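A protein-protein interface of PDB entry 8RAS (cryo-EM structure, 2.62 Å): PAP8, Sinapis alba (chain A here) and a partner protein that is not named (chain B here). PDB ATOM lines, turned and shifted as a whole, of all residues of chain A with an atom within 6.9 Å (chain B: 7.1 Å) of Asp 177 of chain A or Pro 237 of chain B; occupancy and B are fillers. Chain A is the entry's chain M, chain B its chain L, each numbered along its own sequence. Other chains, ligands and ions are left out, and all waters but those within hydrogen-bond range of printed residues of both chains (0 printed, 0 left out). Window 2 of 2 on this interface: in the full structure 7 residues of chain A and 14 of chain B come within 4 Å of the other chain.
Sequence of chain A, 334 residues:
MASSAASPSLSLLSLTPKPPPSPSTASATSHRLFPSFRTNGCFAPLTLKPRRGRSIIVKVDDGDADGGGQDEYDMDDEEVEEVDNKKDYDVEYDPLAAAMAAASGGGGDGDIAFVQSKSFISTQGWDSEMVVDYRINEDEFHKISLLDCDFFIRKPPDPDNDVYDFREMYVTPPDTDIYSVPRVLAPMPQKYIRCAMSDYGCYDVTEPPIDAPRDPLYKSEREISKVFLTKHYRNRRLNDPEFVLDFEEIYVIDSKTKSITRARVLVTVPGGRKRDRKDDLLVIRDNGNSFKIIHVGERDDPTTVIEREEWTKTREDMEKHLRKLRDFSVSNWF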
ATOM      1  N   VAL A 132      18.097  -6.764  28.280  1.00  0.00           N
ATOM      2  CA  VAL A 132      18.708  -6.899  26.976  1.00  0.00           C
ATOM      3  C   VAL A 132      19.498  -5.634  26.663  1.00  0.00           C
ATOM      4  O   VAL A 132      19.363  -4.609  27.325  1.00  0.00           O
ATOM      5  CB  VAL A 132      17.658  -7.196  25.877  1.00  0.00           C
ATOM      6  CG1 VAL A 132      16.724  -8.308  26.325  1.00  0.00           C
ATOM      7  CG2 VAL A 132      16.878  -5.938  25.536  1.00  0.00           C
ATOM      8  N   TYR A 134      19.528  -4.014  23.594  1.00  0.00           N
ATOM      9  CA  TYR A 134      19.051  -3.439  22.345  1.00  0.00           C
ATOM     10  C   TYR A 134      17.605  -2.999  22.516  1.00  0.00           C
ATOM     11  O   TYR A 134      16.896  -3.456  23.417  1.00  0.00           O
ATOM     12  CB  TYR A 134      19.176  -4.428  21.179  1.00  0.00           C
ATOM     13  CG  TYR A 134      18.427  -5.728  21.376  1.00  0.00           C
ATOM     14  CD1 TYR A 134      18.928  -6.726  22.202  1.00  0.00           C
ATOM     15  CD2 TYR A 134      17.218  -5.959  20.732  1.00  0.00           C
ATOM     16  CE1 TYR A 134      18.247  -7.914  22.382  1.00  0.00           C
ATOM     17  CE2 TYR A 134      16.529  -7.144  20.906  1.00  0.00           C
ATOM     18  CZ  TYR A 134      17.049  -8.118  21.733  1.00  0.00           C
ATOM     19  OH  TYR A 134      16.368  -9.299  21.909  1.00  0.00           O
ATOM     20  N   ARG A 135      17.177  -2.097  21.635  1.00  0.00           N
ATOM     21  CA  ARG A 135      15.814  -1.579  21.631  1.00  0.00           C
ATOM     22  C   ARG A 135      15.040  -2.285  20.523  1.00  0.00           C
ATOM     23  O   ARG A 135      15.357  -2.128  19.340  1.00  0.00           O
ATOM     24  CB  ARG A 135      15.810  -0.066  21.428  1.00  0.00           C
ATOM     25  CG  ARG A 135      16.736   0.688  22.367  1.00  0.00           C
ATOM     26  CD  ARG A 135      16.054   1.909  22.961  1.00  0.00           C
ATOM     27  NE  ARG A 135      16.035   3.028  22.028  1.00  0.00           N
ATOM     28  CZ  ARG A 135      16.875   4.053  22.071  1.00  0.00           C
ATOM     29  NH1 ARG A 135      17.822   4.133  22.991  1.00  0.00           N
ATOM     30  NH2 ARG A 135      16.763   5.023  21.167  1.00  0.00           N
ATOM     31  N   ILE A 136      14.026  -3.059  20.906  1.00  0.00           N
ATOM     32  CA  ILE A 136      13.239  -3.823  19.946  1.00  0.00           C
ATOM     33  C   ILE A 136      12.325  -2.881  19.174  1.00  0.00           C
ATOM     34  O   ILE A 136      12.147  -1.719  19.554  1.00  0.00           O
ATOM     35  CB  ILE A 136      12.424  -4.932  20.637  1.00  0.00           C
ATOM     36  CG1 ILE A 136      11.086  -4.379  21.136  1.00  0.00           C
ATOM     37  CG2 ILE A 136      13.217  -5.533  21.786  1.00  0.00           C
ATOM     38  CD1 ILE A 136      10.304  -5.343  21.998  1.00  0.00           C
ATOM     39  N   GLU A 138       8.599  -2.050  18.215  1.00  0.00           N
ATOM     40  CA  GLU A 138       7.285  -2.321  18.781  1.00  0.00           C
ATOM     41  C   GLU A 138       6.194  -2.449  17.728  1.00  0.00           C
ATOM     42  O   GLU A 138       5.046  -2.736  18.083  1.00  0.00           O
ATOM     43  CB  GLU A 138       6.910  -1.225  19.779  1.00  0.00           C
ATOM     44  CG  GLU A 138       7.807  -1.172  21.000  1.00  0.00           C
ATOM     45  CD  GLU A 138       7.323  -0.173  22.030  1.00  0.00           C
ATOM     46  OE1 GLU A 138       6.284   0.475  21.787  1.00  0.00           O
ATOM     47  OE2 GLU A 138       7.982  -0.032  23.081  1.00  0.00           O
ATOM     48  N   THR A 172       8.885  -4.446  30.227  1.00  0.00           N
ATOM     49  CA  THR A 172       9.468  -3.151  30.533  1.00  0.00           C
ATOM     50  C   THR A 172       8.633  -2.455  31.592  1.00  0.00           C
ATOM     51  O   THR A 172       7.438  -2.739  31.739  1.00  0.00           O
ATOM     52  CB  THR A 172       9.548  -2.254  29.287  1.00  0.00           C
ATOM     53  OG1 THR A 172       8.250  -1.723  28.995  1.00  0.00           O
ATOM     54  CG2 THR A 172      10.045  -3.034  28.090  1.00  0.00           C
ATOM     55  N   PRO A 173       9.230  -1.541  32.354  1.00  0.00           N
ATOM     56  CA  PRO A 173       8.425  -0.662  33.191  1.00  0.00           C
ATOM     57  C   PRO A 173       7.536   0.207  32.329  1.00  0.00           C
ATOM     58  O   PRO A 173       7.856   0.482  31.157  1.00  0.00           O
ATOM     59  CB  PRO A 173       9.473   0.167  33.948  1.00  0.00           C
ATOM     60  CG  PRO A 173      10.730   0.024  33.167  1.00  0.00           C
ATOM     61  CD  PRO A 173      10.673  -1.329  32.546  1.00  0.00           C
ATOM     62  N   ASP A 175       5.851   2.640  30.017  1.00  0.00           N
ATOM     63  CA  ASP A 175       6.376   3.720  29.181  1.00  0.00           C
ATOM     64  C   ASP A 175       7.894   3.850  29.337  1.00  0.00           C
ATOM     65  O   ASP A 175       8.421   4.871  29.781  1.00  0.00           O
ATOM     66  CB  ASP A 175       5.670   5.045  29.488  1.00  0.00           C
ATOM     67  CG  ASP A 175       5.585   5.950  28.275  1.00  0.00           C
ATOM     68  OD1 ASP A 175       4.989   5.531  27.262  1.00  0.00           O
ATOM     69  OD2 ASP A 175       6.114   7.079  28.336  1.00  0.00           O
ATOM     70  N   THR A 176       8.593   2.782  28.958  1.00  0.00           N
ATOM     71  CA  THR A 176      10.046   2.748  29.020  1.00  0.00           C
ATOM     72  C   THR A 176      10.557   1.775  27.968  1.00  0.00           C
ATOM     73  O   THR A 176       9.977   0.704  27.773  1.00  0.00           O
ATOM     74  CB  THR A 176      10.539   2.335  30.412  1.00  0.00           C
ATOM     75  OG1 THR A 176       9.996   3.221  31.399  1.00  0.00           O
ATOM     76  CG2 THR A 176      12.053   2.388  30.483  1.00  0.00           C
ATOM     77  N   ASP A 177      11.642   2.155  27.292  1.00  0.00           N
ATOM     78  CA  ASP A 177      12.246   1.336  26.248  1.00  0.00           C
ATOM     79  C   ASP A 177      13.478   0.582  26.737  1.00  0.00           C
ATOM     80  O   ASP A 177      14.400   0.327  25.956  1.00  0.00           O
ATOM     81  CB  ASP A 177      12.595   2.197  25.034  1.00  0.00           C
ATOM     82  CG  ASP A 177      13.177   3.541  25.421  1.00  0.00           C
ATOM     83  OD1 ASP A 177      13.534   3.721  26.604  1.00  0.00           O
ATOM     84  OD2 ASP A 177      13.273   4.422  24.540  1.00  0.00           O
ATOM     85  N   ILE A 178      13.514   0.225  28.016  1.00  0.00           N
ATOM     86  CA  ILE A 178      14.585  -0.599  28.572  1.00  0.00           C
ATOM     87  C   ILE A 178      14.000  -2.001  28.710  1.00  0.00           C
ATOM     88  O   ILE A 178      13.369  -2.345  29.710  1.00  0.00           O
ATOM     89  CB  ILE A 178      15.103  -0.048  29.899  1.00  0.00           C
ATOM     90  CG1 ILE A 178      15.538   1.409  29.731  1.00  0.00           C
ATOM     91  CG2 ILE A 178      16.257  -0.893  30.410  1.00  0.00           C
ATOM     92  CD1 ILE A 178      15.700   2.153  31.038  1.00  0.00           C
ATOM     93  N   TYR A 179      14.221  -2.822  27.689  1.00  0.00           N
ATOM     94  CA  TYR A 179      13.544  -4.104  27.578  1.00  0.00           C
ATOM     95  C   TYR A 179      14.280  -5.185  28.360  1.00  0.00           C
ATOM     96  O   TYR A 179      15.506  -5.158  28.503  1.00  0.00           O
ATOM     97  CB  TYR A 179      13.416  -4.511  26.110  1.00  0.00           C
ATOM     98  CG  TYR A 179      12.687  -3.491  25.262  1.00  0.00           C
ATOM     99  CD1 TYR A 179      13.350  -2.387  24.744  1.00  0.00           C
ATOM    100  CD2 TYR A 179      11.335  -3.629  24.984  1.00  0.00           C
ATOM    101  CE1 TYR A 179      12.688  -1.450  23.974  1.00  0.00           C
ATOM    102  CE2 TYR A 179      10.664  -2.696  24.218  1.00  0.00           C
ATOM    103  CZ  TYR A 179      11.346  -1.611  23.713  1.00  0.00           C
ATOM    104  OH  TYR A 179      10.682  -0.683  22.945  1.00  0.00           O
ATOM    105  N   PRO B 148      12.254  13.713  29.699  1.00  0.00           N
ATOM    106  CA  PRO B 148      13.269  14.294  28.803  1.00  0.00           C
ATOM    107  C   PRO B 148      12.770  15.484  28.002  1.00  0.00           C
ATOM    108  O   PRO B 148      13.593  16.268  27.506  1.00  0.00           O
ATOM    109  CB  PRO B 148      13.645  13.120  27.888  1.00  0.00           C
ATOM    110  CG  PRO B 148      12.501  12.167  27.988  1.00  0.00           C
ATOM    111  CD  PRO B 148      11.956  12.309  29.371  1.00  0.00           C
ATOM    112  N   TRP B 232      16.252  15.561  17.982  1.00  0.00           N
ATOM    113  CA  TRP B 232      15.506  14.361  17.619  1.00  0.00           C
ATOM    114  C   TRP B 232      16.368  13.382  16.833  1.00  0.00           C
ATOM    115  O   TRP B 232      15.944  12.872  15.792  1.00  0.00           O
ATOM    116  CB  TRP B 232      14.254  14.725  16.821  1.00  0.00           C
ATOM    117  CG  TRP B 232      13.013  14.766  17.655  1.00  0.00           C
ATOM    118  CD1 TRP B 232      12.181  13.724  17.935  1.00  0.00           C
ATOM    119  CD2 TRP B 232      12.462  15.909  18.318  1.00  0.00           C
ATOM    120  NE1 TRP B 232      11.146  14.145  18.732  1.00  0.00           N
ATOM    121  CE2 TRP B 232      11.296  15.484  18.983  1.00  0.00           C
ATOM    122  CE3 TRP B 232      12.843  17.251  18.416  1.00  0.00           C
ATOM    123  CZ2 TRP B 232      10.507  16.351  19.732  1.00  0.00           C
ATOM    124  CZ3 TRP B 232      12.058  18.109  19.160  1.00  0.00           C
ATOM    125  CH2 TRP B 232      10.903  17.657  19.809  1.00  0.00           C
ATOM    126  N   HIS B 233      17.576  13.115  17.321  1.00  0.00           N
ATOM    127  CA  HIS B 233      18.501  12.223  16.634  1.00  0.00           C
ATOM    128  C   HIS B 233      18.102  10.767  16.887  1.00  0.00           C
ATOM    129  O   HIS B 233      17.021  10.471  17.404  1.00  0.00           O
ATOM    130  CB  HIS B 233      19.934  12.517  17.068  1.00  0.00           C
ATOM    131  CG  HIS B 233      20.195  12.249  18.517  1.00  0.00           C
ATOM    132  ND1 HIS B 233      20.018  13.205  19.493  1.00  0.00           N
ATOM    133  CD2 HIS B 233      20.628  11.137  19.155  1.00  0.00           C
ATOM    134  CE1 HIS B 233      20.325  12.691  20.671  1.00  0.00           C
ATOM    135  NE2 HIS B 233      20.698  11.437  20.493  1.00  0.00           N
ATOM    136  N   SER B 234      18.979   9.835  16.508  1.00  0.00           N
ATOM    137  CA  SER B 234      18.635   8.417  16.562  1.00  0.00           C
ATOM    138  C   SER B 234      18.464   7.922  17.995  1.00  0.00           C
ATOM    139  O   SER B 234      17.557   7.130  18.277  1.00  0.00           O
ATOM    140  CB  SER B 234      19.705   7.595  15.844  1.00  0.00           C
ATOM    141  OG  SER B 234      20.820   7.367  16.688  1.00  0.00           O
ATOM    142  N   GLY B 235      19.317   8.373  18.909  1.00  0.00           N
ATOM    143  CA  GLY B 235      19.383   7.810  20.241  1.00  0.00           C
ATOM    144  C   GLY B 235      18.349   8.285  21.236  1.00  0.00           C
ATOM    145  O   GLY B 235      18.389   7.855  22.393  1.00  0.00           O
ATOM    146  N   VAL B 236      17.428   9.156  20.837  1.00  0.00           N
ATOM    147  CA  VAL B 236      16.409   9.675  21.746  1.00  0.00           C
ATOM    148  C   VAL B 236      15.488   8.537  22.171  1.00  0.00           C
ATOM    149  O   VAL B 236      15.290   7.583  21.405  1.00  0.00           O
ATOM    150  CB  VAL B 236      15.612  10.819  21.099  1.00  0.00           C
ATOM    151  CG1 VAL B 236      16.519  12.009  20.831  1.00  0.00           C
ATOM    152  CG2 VAL B 236      14.942  10.349  19.820  1.00  0.00           C
ATOM    153  N   PRO B 237      14.923   8.581  23.376  1.00  0.00           N
ATOM    154  CA  PRO B 237      14.004   7.521  23.803  1.00  0.00           C
ATOM    155  C   PRO B 237      12.737   7.510  22.961  1.00  0.00           C
ATOM    156  O   PRO B 237      12.427   8.449  22.225  1.00  0.00           O
ATOM    157  CB  PRO B 237      13.703   7.874  25.263  1.00  0.00           C
ATOM    158  CG  PRO B 237      14.850   8.728  25.690  1.00  0.00           C
ATOM    159  CD  PRO B 237      15.226   9.515  24.471  1.00  0.00           C
ATOM    160  N   LEU B 238      11.999   6.404  23.079  1.00  0.00           N
ATOM    161  CA  LEU B 238      10.803   6.217  22.265  1.00  0.00           C
ATOM    162  C   LEU B 238       9.746   7.270  22.573  1.00  0.00           C
ATOM    163  O   LEU B 238       9.020   7.712  21.674  1.00  0.00           O
ATOM    164  CB  LEU B 238      10.240   4.812  22.481  1.00  0.00           C
ATOM    165  CG  LEU B 238       9.086   4.393  21.570  1.00  0.00           C
ATOM    166  CD1 LEU B 238       9.379   4.755  20.125  1.00  0.00           C
ATOM    167  CD2 LEU B 238       8.821   2.907  21.707  1.00  0.00           C
ATOM    168  N   LYS B 239       9.642   7.686  23.837  1.00  0.00           N
ATOM    169  CA  LYS B 239       8.650   8.689  24.210  1.00  0.00           C
ATOM    170  C   LYS B 239       8.935  10.048  23.584  1.00  0.00           C
ATOM    171  O   LYS B 239       8.026  10.882  23.509  1.00  0.00           O
ATOM    172  CB  LYS B 239       8.577   8.820  25.731  1.00  0.00           C
ATOM    173  CG  LYS B 239       9.907   9.114  26.397  1.00  0.00           C
ATOM    174  CD  LYS B 239       9.706   9.591  27.825  1.00  0.00           C
ATOM    175  CE  LYS B 239       9.067   8.513  28.682  1.00  0.00           C
ATOM    176  NZ  LYS B 239      10.068   7.523  29.160  1.00  0.00           N
ATOM    177  N   ILE B 240      10.164  10.290  23.140  1.00  0.00           N
ATOM    178  CA  ILE B 240      10.520  11.529  22.463  1.00  0.00           C
ATOM    179  C   ILE B 240      10.444  11.382  20.949  1.00  0.00           C
ATOM    180  O   ILE B 240       9.996  12.297  20.257  1.00  0.00           O
ATOM    181  CB  ILE B 240      11.923  11.992  22.906  1.00  0.00           C
ATOM    182  CG1 ILE B 240      11.950  12.240  24.415  1.00  0.00           C
ATOM    183  CG2 ILE B 240      12.338  13.243  22.154  1.00  0.00           C
ATOM    184  CD1 ILE B 240      11.169  13.461  24.841  1.00  0.00           C
ATOM    185  N   LYS B 241      10.873  10.233  20.421  1.00  0.00           N
ATOM    186  CA  LYS B 241      10.852  10.025  18.977  1.00  0.00           C
ATOM    187  C   LYS B 241       9.429  10.049  18.434  1.00  0.00           C
ATOM    188  O   LYS B 241       9.184  10.562  17.335  1.00  0.00           O
ATOM    189  CB  LYS B 241      11.537   8.706  18.626  1.00  0.00           C
ATOM    190  CG  LYS B 241      11.654   8.446  17.134  1.00  0.00           C
ATOM    191  CD  LYS B 241      12.076   7.015  16.855  1.00  0.00           C
ATOM    192  CE  LYS B 241      13.487   6.750  17.357  1.00  0.00           C
ATOM    193  NZ  LYS B 241      14.506   7.522  16.594  1.00  0.00           N
ATOM    194  N   ARG B 242       8.475   9.498  19.186  1.00  0.00           N
ATOM    195  CA  ARG B 242       7.093   9.475  18.724  1.00  0.00           C
ATOM    196  C   ARG B 242       6.442  10.852  18.768  1.00  0.00           C
ATOM    197  O   ARG B 242       5.402  11.048  18.131  1.00  0.00           O
ATOM    198  CB  ARG B 242       6.276   8.480  19.549  1.00  0.00           C
ATOM    199  CG  ARG B 242       6.005   8.915  20.977  1.00  0.00           C
ATOM    200  CD  ARG B 242       5.028   7.971  21.655  1.00  0.00           C
ATOM    201  NE  ARG B 242       4.755   8.356  23.033  1.00  0.00           N
ATOM    202  CZ  ARG B 242       5.127   7.654  24.095  1.00  0.00           C
ATOM    203  NH1 ARG B 242       5.795   6.519  23.973  1.00  0.00           N
ATOM    204  NH2 ARG B 242       4.820   8.101  25.309  1.00  0.00           N
ATOM    205  N   LEU B 243       7.020  11.802  19.506  1.00  0.00           N
ATOM    206  CA  LEU B 243       6.492  13.163  19.498  1.00  0.00           C
ATOM    207  C   LEU B 243       6.607  13.787  18.114  1.00  0.00           C
ATOM    208  O   LEU B 243       5.675  14.448  17.642  1.00  0.00           O
ATOM    209  CB  LEU B 243       7.222  14.019  20.531  1.00  0.00           C
ATOM    210  CG  LEU B 243       7.044  13.638  22.000  1.00  0.00           C
ATOM    211  CD1 LEU B 243       7.865  14.553  22.891  1.00  0.00           C
ATOM    212  CD2 LEU B 243       5.580  13.690  22.385  1.00  0.00           C
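NH2 of Arg 135 of chain A lies within hydrogen-bond range of O of Gly 235 of chain B, at 3.5 Å.
The guanidinium group (NH2) of Arg 242 of chain B is in salt-bridge range of the side-chain carboxylate (OD1) of Asp 175 of chain A (3.2 Å).
The side-chain amino group of Lys 239 of chain B is in hydrogen-bond range of the backbone carbonyl oxygen of Asp 175 of chain A.
The backbone carbonyl oxygen (O) of Val 236 of chain B lies within hydrogen-bond range of the guanidinium group (NH2) of Arg 135 of chain A.
The side-chain carboxylate (OD2) of Asp 177 of chain A is in hydrogen-bond range of the backbone NH (N) of Leu 238 of chain B (2.8 Å).
Of the 12 printed residues of chain A, 4 touch a printed residue of chain B.
Among the printed residues, Asp or Glu carboxylates within 4 Å of a Lys or Arg side-chain nitrogen of the other chain: Asp 175 of chain A with Arg 242 of chain B.
Of chain A, only Asp 177 comes within 4 Å of Pro 237 of chain B.
Printed residues of chain B within 4 Å of Arg 135 of chain A: Ser 234 (3.7 Å), Gly 235 (3.5 Å) and Val 236 (3.0 Å).
Of the printed residues of chain A, Val 236 of chain B touches Arg 135.
Of the printed residues of chain B, Asp 175 of chain A touches Lys 239 (3.2 Å) and Arg 242 (3.2 Å).
Printed residues of chain A within 4 Å of Lys 239 of chain B: Asp 175 (3.2 Å).
Tyr 134 of chain A touches none of the printed residues of chain B.
The nearest residue of chain B that does not touch Asp 177 of chain A is Val 236 of chain B (4.9 Å).
OE2 of Glu 138 of chain A sits at hydrogen-bond distance from OH of Tyr 179 of chain A.
NE of Arg 135 of chain A lies within salt-bridge range of OD2 of Asp 177 of chain A (3.99 Å).
O of Ser 234 of chain B touches NH2 of Arg 135 of chain A (3.7 Å).
Leu 238 of chain B touches Glu 138 of chain A (CD2 to OE2, 3.4 Å).
Pro 237 of chain B touches Asp 177 of chain A.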
